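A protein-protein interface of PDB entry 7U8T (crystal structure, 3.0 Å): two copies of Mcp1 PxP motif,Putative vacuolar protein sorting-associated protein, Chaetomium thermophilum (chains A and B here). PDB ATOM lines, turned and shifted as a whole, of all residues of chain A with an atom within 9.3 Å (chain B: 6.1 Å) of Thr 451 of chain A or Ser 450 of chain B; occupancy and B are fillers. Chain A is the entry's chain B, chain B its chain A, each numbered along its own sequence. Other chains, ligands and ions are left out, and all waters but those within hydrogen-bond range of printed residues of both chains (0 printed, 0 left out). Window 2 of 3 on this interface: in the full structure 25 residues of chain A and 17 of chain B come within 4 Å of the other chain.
N of Thr 451 of chain B sits at hydrogen-bond distance from O of Thr 451 of chain A, 3.0 Å away. The backbone NH of Glu 453 of chain A lies within hydrogen-bond range of the backbone carbonyl oxygen of Gly 449 of chain B, at 3.1 Å.
The backbone NH (N) of Gly 449 of chain A lies within hydrogen-bond range of the backbone carbonyl oxygen (O) of Val 471 of chain A, 2.7 Å away. The side-chain hydroxyl of Ser 450 of chain A sits at hydrogen-bond distance from the backbone carbonyl oxygen of Ala 447 of chain A, 2.9 Å away. The backbone carbonyl oxygen (O) of Val 471 of chain B lies within hydrogen-bond range of the backbone NH (N) of Gly 449 of chain B (2.7 Å). O of Ala 447 of chain B sits at hydrogen-bond distance from OG of Ser 450 of chain B. The backbone NH (N) of Val 469 of chain A is in hydrogen-bond range of the backbone carbonyl oxygen (O) of Thr 452 of chain A, 2.9 Å away. N of Val 471 of chain A is in hydrogen-bond range of O of Ser 450 of chain A (2.9 Å).
Among the printed residues, pairs that only touch across the chains: Gly 449 of chain A with Thr 452 of chain B (3.9 Å), Ser 450 of chain A with Thr 451 of chain B (3.3 Å), Thr 451 of chain A with Ser 450 of chain B (3.4 Å), Thr 452 of chain A with Gly 449 of chain B (3.7 Å) and Glu 453 of chain A with Ile 448 of chain B (3.9 Å).
Thr 451 of chain A touches just these residues of chain B: Ser 450 (3.4 Å) and Thr 451 (2.4 Å). Ser 450 of chain B touches one residue of chain A. No residue of chain A comes within 4 Å of Ala 447 of chain B. Of chain A, only Thr 452 (3.7 Å) and Glu 453 (3.1 Å) come within 4 Å of Gly 449 of chain B. Of chain A, only Ser 450 (3.3 Å) and Thr 451 (2.4 Å) come within 4 Å of Thr 451 of chain B. No residue of chain A comes within 4 Å of Thr 470 of chain B. No residue of chain A comes within 4 Å of Val 471 of chain B. Of the printed residues of chain B, Ser 450 of chain A touches Thr 451. Of the printed residues of chain A, Ile 448 of chain B touches Glu 453 (3.9 Å). Of the printed residues of chain B, Glu 453 of chain A touches Ile 448 (3.9 Å) and Gly 449 (3.1 Å). Met 575 of chain A touches none of the printed residues of chain B. Ala 447 of chain A touches none of the printed residues of chain B. The nearest residue of chain B that does not touch Thr 451 of chain A is Gly 449 of chain B (4.04 Å). The nearest residue of chain A that does not touch Ser 450 of chain B is Thr 452 of chain A (4.1 Å). The nearest printed residue of chain B that does not touch Gly 449 of chain A is Thr 451 of chain B (4.2 Å).
Of the 24 printed residues of chain A, 5 touch a printed residue of chain B. Among the printed residues, no Asp or Glu carboxylate lies within 4 Å of a Lys or Arg side-chain nitrogen of the other chain.
Gly 449 of chain A touches Thr 452 of chain B, and with the chains exchanged Thr 452 of chain A touches Gly 449 of chain B. Ser 450 of chain A touches Thr 451 of chain B, and with the chains exchanged Thr 451 of chain A touches Ser 450 of chain B. Thr 451 of chain A touches its own counterpart, Thr 451 of chain B. Positions printed for both chains: 444, 447, 448, 449, 450, 451, 452, 469, 470, 471 and 472. Of the 7 pairs that touch across the chains among the printed residues, 5 have their exchanged pair printed and touching as well.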
ATOM      1  N   GLN A 443     -21.447 -38.394   1.203  1.00  0.00           N
ATOM      2  CA  GLN A 443     -21.907 -37.027   1.018  1.00  0.00           C
ATOM      3  C   GLN A 443     -22.940 -36.973  -0.100  1.00  0.00           C
ATOM      4  O   GLN A 443     -22.850 -37.705  -1.091  1.00  0.00           O
ATOM      5  CB  GLN A 443     -20.745 -36.085   0.680  1.00  0.00           C
ATOM      6  CG  GLN A 443     -19.618 -36.090   1.697  1.00  0.00           C
ATOM      7  CD  GLN A 443     -20.092 -35.793   3.104  1.00  0.00           C
ATOM      8  OE1 GLN A 443     -20.873 -34.866   3.333  1.00  0.00           O
ATOM      9  NE2 GLN A 443     -19.644 -36.601   4.053  1.00  0.00           N
ATOM     10  N   SER A 444     -23.917 -36.091   0.069  1.00  0.00           N
ATOM     11  CA  SER A 444     -24.974 -35.902  -0.912  1.00  0.00           C
ATOM     12  C   SER A 444     -24.601 -34.766  -1.852  1.00  0.00           C
ATOM     13  O   SER A 444     -24.258 -33.667  -1.404  1.00  0.00           O
ATOM     14  CB  SER A 444     -26.307 -35.604  -0.226  1.00  0.00           C
ATOM     15  OG  SER A 444     -27.227 -35.024  -1.136  1.00  0.00           O
ATOM     16  N   ALA A 447     -28.265 -32.381  -2.381  1.00  0.00           N
ATOM     17  CA  ALA A 447     -28.758 -31.397  -1.415  1.00  0.00           C
ATOM     18  C   ALA A 447     -28.629 -29.962  -1.913  1.00  0.00           C
ATOM     19  O   ALA A 447     -27.627 -29.287  -1.673  1.00  0.00           O
ATOM     20  CB  ALA A 447     -28.028 -31.600  -0.093  1.00  0.00           C
ATOM     21  N   ILE A 448     -29.669 -29.496  -2.609  1.00  0.00           N
ATOM     22  CA  ILE A 448     -29.663 -28.192  -3.267  1.00  0.00           C
ATOM     23  C   ILE A 448     -29.688 -27.087  -2.220  1.00  0.00           C
ATOM     24  O   ILE A 448     -30.567 -27.055  -1.351  1.00  0.00           O
ATOM     25  CB  ILE A 448     -30.848 -28.071  -4.239  1.00  0.00           C
ATOM     26  CG1 ILE A 448     -30.577 -28.885  -5.500  1.00  0.00           C
ATOM     27  CG2 ILE A 448     -31.116 -26.615  -4.636  1.00  0.00           C
ATOM     28  CD1 ILE A 448     -29.299 -28.483  -6.189  1.00  0.00           C
ATOM     29  N   GLY A 449     -28.714 -26.183  -2.299  1.00  0.00           N
ATOM     30  CA  GLY A 449     -28.611 -25.084  -1.364  1.00  0.00           C
ATOM     31  C   GLY A 449     -28.172 -25.561   0.003  1.00  0.00           C
ATOM     32  O   GLY A 449     -28.907 -25.402   0.986  1.00  0.00           O
ATOM     33  N   SER A 450     -26.990 -26.168   0.085  1.00  0.00           N
ATOM     34  CA  SER A 450     -26.515 -26.644   1.376  1.00  0.00           C
ATOM     35  C   SER A 450     -25.024 -26.399   1.513  1.00  0.00           C
ATOM     36  O   SER A 450     -24.275 -26.491   0.536  1.00  0.00           O
ATOM     37  CB  SER A 450     -26.801 -28.139   1.596  1.00  0.00           C
ATOM     38  OG  SER A 450     -26.010 -28.949   0.746  1.00  0.00           O
ATOM     39  N   THR A 451     -24.605 -26.080   2.735  1.00  0.00           N
ATOM     40  CA  THR A 451     -23.201 -25.971   3.103  1.00  0.00           C
ATOM     41  C   THR A 451     -22.949 -26.918   4.265  1.00  0.00           C
ATOM     42  O   THR A 451     -23.547 -26.763   5.334  1.00  0.00           O
ATOM     43  CB  THR A 451     -22.831 -24.537   3.490  1.00  0.00           C
ATOM     44  OG1 THR A 451     -23.645 -24.108   4.588  1.00  0.00           O
ATOM     45  CG2 THR A 451     -23.005 -23.583   2.314  1.00  0.00           C
ATOM     46  N   THR A 452     -22.095 -27.915   4.049  1.00  0.00           N
ATOM     47  CA  THR A 452     -21.729 -28.853   5.104  1.00  0.00           C
ATOM     48  C   THR A 452     -20.230 -28.783   5.385  1.00  0.00           C
ATOM     49  O   THR A 452     -19.432 -28.378   4.534  1.00  0.00           O
ATOM     50  CB  THR A 452     -22.114 -30.303   4.756  1.00  0.00           C
ATOM     51  OG1 THR A 452     -21.068 -30.904   3.984  1.00  0.00           O
ATOM     52  CG2 THR A 452     -23.440 -30.378   3.990  1.00  0.00           C
ATOM     53  N   GLU A 453     -19.860 -29.177   6.604  1.00  0.00           N
ATOM     54  CA  GLU A 453     -18.460 -29.275   7.011  1.00  0.00           C
ATOM     55  C   GLU A 453     -18.045 -30.740   7.021  1.00  0.00           C
ATOM     56  O   GLU A 453     -18.700 -31.571   7.659  1.00  0.00           O
ATOM     57  CB  GLU A 453     -18.227 -28.661   8.393  1.00  0.00           C
ATOM     58  CG  GLU A 453     -16.756 -28.666   8.820  1.00  0.00           C
ATOM     59  CD  GLU A 453     -16.522 -28.054  10.194  1.00  0.00           C
ATOM     60  OE1 GLU A 453     -17.505 -27.674  10.865  1.00  0.00           O
ATOM     61  OE2 GLU A 453     -15.345 -27.940  10.596  1.00  0.00           O
ATOM     62  N   VAL A 454     -16.959 -31.053   6.317  1.00  0.00           N
ATOM     63  CA  VAL A 454     -16.464 -32.419   6.188  1.00  0.00           C
ATOM     64  C   VAL A 454     -15.078 -32.492   6.817  1.00  0.00           C
ATOM     65  O   VAL A 454     -14.152 -31.801   6.379  1.00  0.00           O
ATOM     66  CB  VAL A 454     -16.428 -32.872   4.722  1.00  0.00           C
ATOM     67  CG1 VAL A 454     -15.807 -34.248   4.619  1.00  0.00           C
ATOM     68  CG2 VAL A 454     -17.829 -32.890   4.155  1.00  0.00           C
ATOM     69  N   LEU A 467     -12.943 -29.340   5.454  1.00  0.00           N
ATOM     70  CA  LEU A 467     -13.410 -28.857   4.167  1.00  0.00           C
ATOM     71  C   LEU A 467     -14.844 -28.356   4.276  1.00  0.00           C
ATOM     72  O   LEU A 467     -15.617 -28.810   5.124  1.00  0.00           O
ATOM     73  CB  LEU A 467     -13.340 -29.960   3.111  1.00  0.00           C
ATOM     74  CG  LEU A 467     -11.947 -30.482   2.784  1.00  0.00           C
ATOM     75  CD1 LEU A 467     -12.049 -31.639   1.814  1.00  0.00           C
ATOM     76  CD2 LEU A 467     -11.079 -29.373   2.218  1.00  0.00           C
ATOM     77  N   GLY A 468     -15.185 -27.411   3.402  1.00  0.00           N
ATOM     78  CA  GLY A 468     -16.548 -26.947   3.252  1.00  0.00           C
ATOM     79  C   GLY A 468     -17.109 -27.332   1.897  1.00  0.00           C
ATOM     80  O   GLY A 468     -16.512 -27.027   0.858  1.00  0.00           O
ATOM     81  N   VAL A 469     -18.248 -28.019   1.895  1.00  0.00           N
ATOM     82  CA  VAL A 469     -18.886 -28.498   0.675  1.00  0.00           C
ATOM     83  C   VAL A 469     -20.174 -27.712   0.475  1.00  0.00           C
ATOM     84  O   VAL A 469     -21.092 -27.790   1.302  1.00  0.00           O
ATOM     85  CB  VAL A 469     -19.170 -30.005   0.739  1.00  0.00           C
ATOM     86  CG1 VAL A 469     -19.768 -30.489  -0.572  1.00  0.00           C
ATOM     87  CG2 VAL A 469     -17.899 -30.764   1.073  1.00  0.00           C
ATOM     88  N   THR A 470     -20.245 -26.962  -0.624  1.00  0.00           N
ATOM     89  CA  THR A 470     -21.421 -26.165  -0.959  1.00  0.00           C
ATOM     90  C   THR A 470     -22.061 -26.723  -2.224  1.00  0.00           C
ATOM     91  O   THR A 470     -21.411 -26.800  -3.268  1.00  0.00           O
ATOM     92  CB  THR A 470     -21.055 -24.692  -1.145  1.00  0.00           C
ATOM     93  OG1 THR A 470     -20.524 -24.168   0.078  1.00  0.00           O
ATOM     94  CG2 THR A 470     -22.280 -23.879  -1.543  1.00  0.00           C
ATOM     95  N   VAL A 471     -23.329 -27.106  -2.135  1.00  0.00           N
ATOM     96  CA  VAL A 471     -24.066 -27.633  -3.279  1.00  0.00           C
ATOM     97  C   VAL A 471     -25.205 -26.675  -3.611  1.00  0.00           C
ATOM     98  O   VAL A 471     -26.089 -26.431  -2.774  1.00  0.00           O
ATOM     99  CB  VAL A 471     -24.591 -29.051  -3.012  1.00  0.00           C
ATOM    100  CG1 VAL A 471     -25.423 -29.535  -4.198  1.00  0.00           C
ATOM    101  CG2 VAL A 471     -23.437 -30.004  -2.737  1.00  0.00           C
ATOM    102  N   ASP A 472     -25.176 -26.141  -4.839  1.00  0.00           N
ATOM    103  CA  ASP A 472     -26.167 -25.204  -5.367  1.00  0.00           C
ATOM    104  C   ASP A 472     -26.621 -25.641  -6.756  1.00  0.00           C
ATOM    105  O   ASP A 472     -26.048 -26.542  -7.371  1.00  0.00           O
ATOM    106  CB  ASP A 472     -25.610 -23.775  -5.454  1.00  0.00           C
ATOM    107  CG  ASP A 472     -25.519 -23.097  -4.109  1.00  0.00           C
ATOM    108  OD1 ASP A 472     -26.199 -23.549  -3.167  1.00  0.00           O
ATOM    109  OD2 ASP A 472     -24.752 -22.116  -3.986  1.00  0.00           O
ATOM    110  N   THR A 485     -19.130 -27.114  -4.912  1.00  0.00           N
ATOM    111  CA  THR A 485     -17.876 -26.452  -4.589  1.00  0.00           C
ATOM    112  C   THR A 485     -17.244 -27.144  -3.388  1.00  0.00           C
ATOM    113  O   THR A 485     -17.879 -27.273  -2.332  1.00  0.00           O
ATOM    114  CB  THR A 485     -18.104 -24.971  -4.284  1.00  0.00           C
ATOM    115  OG1 THR A 485     -18.767 -24.345  -5.391  1.00  0.00           O
ATOM    116  CG2 THR A 485     -16.778 -24.266  -4.031  1.00  0.00           C
ATOM    117  N   ALA A 487     -14.229 -26.460  -0.880  1.00  0.00           N
ATOM    118  CA  ALA A 487     -13.475 -25.311  -0.411  1.00  0.00           C
ATOM    119  C   ALA A 487     -12.781 -25.688   0.890  1.00  0.00           C
ATOM    120  O   ALA A 487     -13.155 -26.678   1.529  1.00  0.00           O
ATOM    121  CB  ALA A 487     -14.427 -24.124  -0.197  1.00  0.00           C
ATOM    122  N   ARG A 489     -12.386 -25.086   4.848  1.00  0.00           N
ATOM    123  CA  ARG A 489     -13.285 -24.558   5.867  1.00  0.00           C
ATOM    124  C   ARG A 489     -12.759 -23.246   6.435  1.00  0.00           C
ATOM    125  O   ARG A 489     -13.547 -22.349   6.748  1.00  0.00           O
ATOM    126  CB  ARG A 489     -13.480 -25.596   6.978  1.00  0.00           C
ATOM    127  CG  ARG A 489     -14.494 -25.223   8.061  1.00  0.00           C
ATOM    128  CD  ARG A 489     -15.842 -24.881   7.461  1.00  0.00           C
ATOM    129  NE  ARG A 489     -16.909 -24.860   8.457  1.00  0.00           N
ATOM    130  CZ  ARG A 489     -18.192 -24.677   8.170  1.00  0.00           C
ATOM    131  NH1 ARG A 489     -18.601 -24.489   6.925  1.00  0.00           N
ATOM    132  NH2 ARG A 489     -19.086 -24.685   9.154  1.00  0.00           N
ATOM    133  N   MET A 575     -18.145 -15.732   7.500  1.00  0.00           N
ATOM    134  CA  MET A 575     -18.420 -16.962   6.711  1.00  0.00           C
ATOM    135  C   MET A 575     -18.974 -16.618   5.325  1.00  0.00           C
ATOM    136  O   MET A 575     -20.039 -15.975   5.259  1.00  0.00           O
ATOM    137  CB  MET A 575     -19.430 -17.853   7.440  1.00  0.00           C
ATOM    138  CG  MET A 575     -19.687 -19.167   6.729  1.00  0.00           C
ATOM    139  SD  MET A 575     -20.792 -20.252   7.664  1.00  0.00           S
ATOM    140  CE  MET A 575     -19.656 -20.891   8.894  1.00  0.00           C
ATOM    141  N   GLU A 576     -18.271 -17.031   4.265  1.00  0.00           N
ATOM    142  CA  GLU A 576     -18.715 -16.726   2.879  1.00  0.00           C
ATOM    143  C   GLU A 576     -19.720 -17.790   2.428  1.00  0.00           C
ATOM    144  O   GLU A 576     -20.901 -17.439   2.243  1.00  0.00           O
ATOM    145  CB  GLU A 576     -17.528 -16.423   1.960  1.00  0.00           C
ATOM    146  CG  GLU A 576     -17.923 -16.029   0.550  1.00  0.00           C
ATOM    147  CD  GLU A 576     -18.276 -17.200  -0.352  1.00  0.00           C
ATOM    148  OE1 GLU A 576     -17.789 -18.316  -0.085  1.00  0.00           O
ATOM    149  OE2 GLU A 576     -19.044 -16.994  -1.311  1.00  0.00           O
ATOM    150  N   ASP A 577     -19.270 -19.040   2.275  1.00  0.00           N
ATOM    151  CA  ASP A 577     -20.097 -20.209   1.960  1.00  0.00           C
ATOM    152  C   ASP A 577     -19.223 -21.453   2.259  1.00  0.00           C
ATOM    153  O   ASP A 577     -18.241 -21.689   1.528  1.00  0.00           O
ATOM    154  CB  ASP A 577     -20.583 -20.197   0.509  1.00  0.00           C
ATOM    155  CG  ASP A 577     -19.464 -20.372  -0.501  1.00  0.00           C
ATOM    156  OD1 ASP A 577     -18.333 -20.673  -0.072  1.00  0.00           O
ATOM    157  OD2 ASP A 577     -19.734 -20.213  -1.707  1.00  0.00           O
ATOM    158  N   ALA A 578     -19.502 -22.110   3.388  1.00  0.00           N
ATOM    159  CA  ALA A 578     -18.581 -23.154   3.895  1.00  0.00           C
ATOM    160  C   ALA A 578     -17.103 -22.762   3.995  1.00  0.00           C
ATOM    161  O   ALA A 578     -16.249 -23.669   4.017  1.00  0.00           O
ATOM    162  CB  ALA A 578     -18.785 -24.400   3.069  1.00  0.00           C
ATOM    163  N   THR A 579     -16.821 -21.454   4.051  1.00  0.00           N
ATOM    164  CA  THR A 579     -15.418 -20.963   4.122  1.00  0.00           C
ATOM    165  C   THR A 579     -15.335 -19.795   5.106  1.00  0.00           C
ATOM    166  O   THR A 579     -15.817 -18.698   4.762  1.00  0.00           O
ATOM    167  CB  THR A 579     -14.891 -20.564   2.740  1.00  0.00           C
ATOM    168  OG1 THR A 579     -15.261 -21.581   1.808  1.00  0.00           O
ATOM    169  CG2 THR A 579     -13.389 -20.377   2.724  1.00  0.00           C
ATOM    170  N   SER B 444     -31.589 -35.193   7.153  1.00  0.00           N
ATOM    171  CA  SER B 444     -30.599 -35.844   8.004  1.00  0.00           C
ATOM    172  C   SER B 444     -30.244 -34.935   9.174  1.00  0.00           C
ATOM    173  O   SER B 444     -29.777 -33.810   8.972  1.00  0.00           O
ATOM    174  CB  SER B 444     -29.341 -36.192   7.214  1.00  0.00           C
ATOM    175  OG  SER B 444     -28.232 -36.297   8.091  1.00  0.00           O
ATOM    176  N   ALA B 447     -25.644 -34.860  10.168  1.00  0.00           N
ATOM    177  CA  ALA B 447     -24.551 -34.093   9.578  1.00  0.00           C
ATOM    178  C   ALA B 447     -24.176 -32.942  10.503  1.00  0.00           C
ATOM    179  O   ALA B 447     -24.912 -31.956  10.613  1.00  0.00           O
ATOM    180  CB  ALA B 447     -24.953 -33.579   8.199  1.00  0.00           C
ATOM    181  N   ILE B 448     -23.031 -33.063  11.165  1.00  0.00           N
ATOM    182  CA  ILE B 448     -22.603 -32.081  12.155  1.00  0.00           C
ATOM    183  C   ILE B 448     -21.997 -30.874  11.452  1.00  0.00           C
ATOM    184  O   ILE B 448     -21.023 -31.001  10.702  1.00  0.00           O
ATOM    185  CB  ILE B 448     -21.608 -32.697  13.147  1.00  0.00           C
ATOM    186  CG1 ILE B 448     -22.288 -33.820  13.926  1.00  0.00           C
ATOM    187  CG2 ILE B 448     -21.069 -31.640  14.090  1.00  0.00           C
ATOM    188  CD1 ILE B 448     -23.520 -33.346  14.662  1.00  0.00           C
ATOM    189  N   GLY B 449     -22.560 -29.698  11.714  1.00  0.00           N
ATOM    190  CA  GLY B 449     -22.079 -28.479  11.103  1.00  0.00           C
ATOM    191  C   GLY B 449     -22.628 -28.311   9.705  1.00  0.00           C
ATOM    192  O   GLY B 449     -21.870 -28.124   8.747  1.00  0.00           O
ATOM    193  N   SER B 450     -23.949 -28.386   9.567  1.00  0.00           N
ATOM    194  CA  SER B 450     -24.548 -28.311   8.241  1.00  0.00           C
ATOM    195  C   SER B 450     -25.740 -27.370   8.256  1.00  0.00           C
ATOM    196  O   SER B 450     -26.506 -27.338   9.224  1.00  0.00           O
ATOM    197  CB  SER B 450     -24.969 -29.701   7.738  1.00  0.00           C
ATOM    198  OG  SER B 450     -26.117 -30.172   8.421  1.00  0.00           O
ATOM    199  N   THR B 451     -25.865 -26.585   7.183  1.00  0.00           N
ATOM    200  CA  THR B 451     -27.012 -25.719   6.937  1.00  0.00           C
ATOM    201  C   THR B 451     -27.674 -26.165   5.643  1.00  0.00           C
ATOM    202  O   THR B 451     -26.989 -26.390   4.641  1.00  0.00           O
ATOM    203  CB  THR B 451     -26.606 -24.242   6.836  1.00  0.00           C
ATOM    204  OG1 THR B 451     -25.710 -24.050   5.735  1.00  0.00           O
ATOM    205  CG2 THR B 451     -25.944 -23.769   8.111  1.00  0.00           C
ATOM    206  N   THR B 452     -28.996 -26.289   5.661  1.00  0.00           N
ATOM    207  CA  THR B 452     -29.731 -26.866   4.543  1.00  0.00           C
ATOM    208  C   THR B 452     -31.003 -26.070   4.301  1.00  0.00           C
ATOM    209  O   THR B 452     -31.744 -25.783   5.245  1.00  0.00           O
ATOM    210  CB  THR B 452     -30.069 -28.342   4.821  1.00  0.00           C
ATOM    211  OG1 THR B 452     -28.863 -29.059   5.117  1.00  0.00           O
ATOM    212  CG2 THR B 452     -30.744 -28.996   3.619  1.00  0.00           C
ATOM    213  N   VAL B 469     -32.381 -25.145   7.992  1.00  0.00           N
ATOM    214  CA  VAL B 469     -32.124 -26.136   9.031  1.00  0.00           C
ATOM    215  C   VAL B 469     -30.628 -26.143   9.303  1.00  0.00           C
ATOM    216  O   VAL B 469     -29.827 -26.380   8.391  1.00  0.00           O
ATOM    217  CB  VAL B 469     -32.632 -27.525   8.617  1.00  0.00           C
ATOM    218  CG1 VAL B 469     -32.356 -28.550   9.716  1.00  0.00           C
ATOM    219  CG2 VAL B 469     -34.119 -27.460   8.309  1.00  0.00           C
ATOM    220  N   THR B 470     -30.249 -25.868  10.550  1.00  0.00           N
ATOM    221  CA  THR B 470     -28.863 -25.971  10.996  1.00  0.00           C
ATOM    222  C   THR B 470     -28.755 -27.154  11.946  1.00  0.00           C
ATOM    223  O   THR B 470     -29.610 -27.332  12.816  1.00  0.00           O
ATOM    224  CB  THR B 470     -28.405 -24.678  11.685  1.00  0.00           C
ATOM    225  OG1 THR B 470     -28.586 -23.575  10.790  1.00  0.00           O
ATOM    226  CG2 THR B 470     -26.936 -24.739  12.068  1.00  0.00           C
ATOM    227  N   VAL B 471     -27.747 -27.995  11.746  1.00  0.00           N
ATOM    228  CA  VAL B 471     -27.425 -29.056  12.696  1.00  0.00           C
ATOM    229  C   VAL B 471     -25.993 -28.839  13.164  1.00  0.00           C
ATOM    230  O   VAL B 471     -25.062 -28.818  12.343  1.00  0.00           O
ATOM    231  CB  VAL B 471     -27.610 -30.456  12.091  1.00  0.00           C
ATOM    232  CG1 VAL B 471     -27.183 -31.512  13.089  1.00  0.00           C
ATOM    233  CG2 VAL B 471     -29.069 -30.675  11.677  1.00  0.00           C
ATOM    234  N   ASP B 472     -25.828 -28.649  14.478  1.00  0.00           N
ATOM    235  CA  ASP B 472     -24.527 -28.463  15.119  1.00  0.00           C
ATOM    236  C   ASP B 472     -24.382 -29.430  16.291  1.00  0.00           C
ATOM    237  O   ASP B 472     -25.327 -30.114  16.691  1.00  0.00           O
ATOM    238  CB  ASP B 472     -24.340 -27.018  15.625  1.00  0.00           C
ATOM    239  CG  ASP B 472     -24.086 -26.020  14.502  1.00  0.00           C
ATOM    240  OD1 ASP B 472     -23.727 -26.448  13.388  1.00  0.00           O
ATOM    241  OD2 ASP B 472     -24.260 -24.802  14.731  1.00  0.00           O
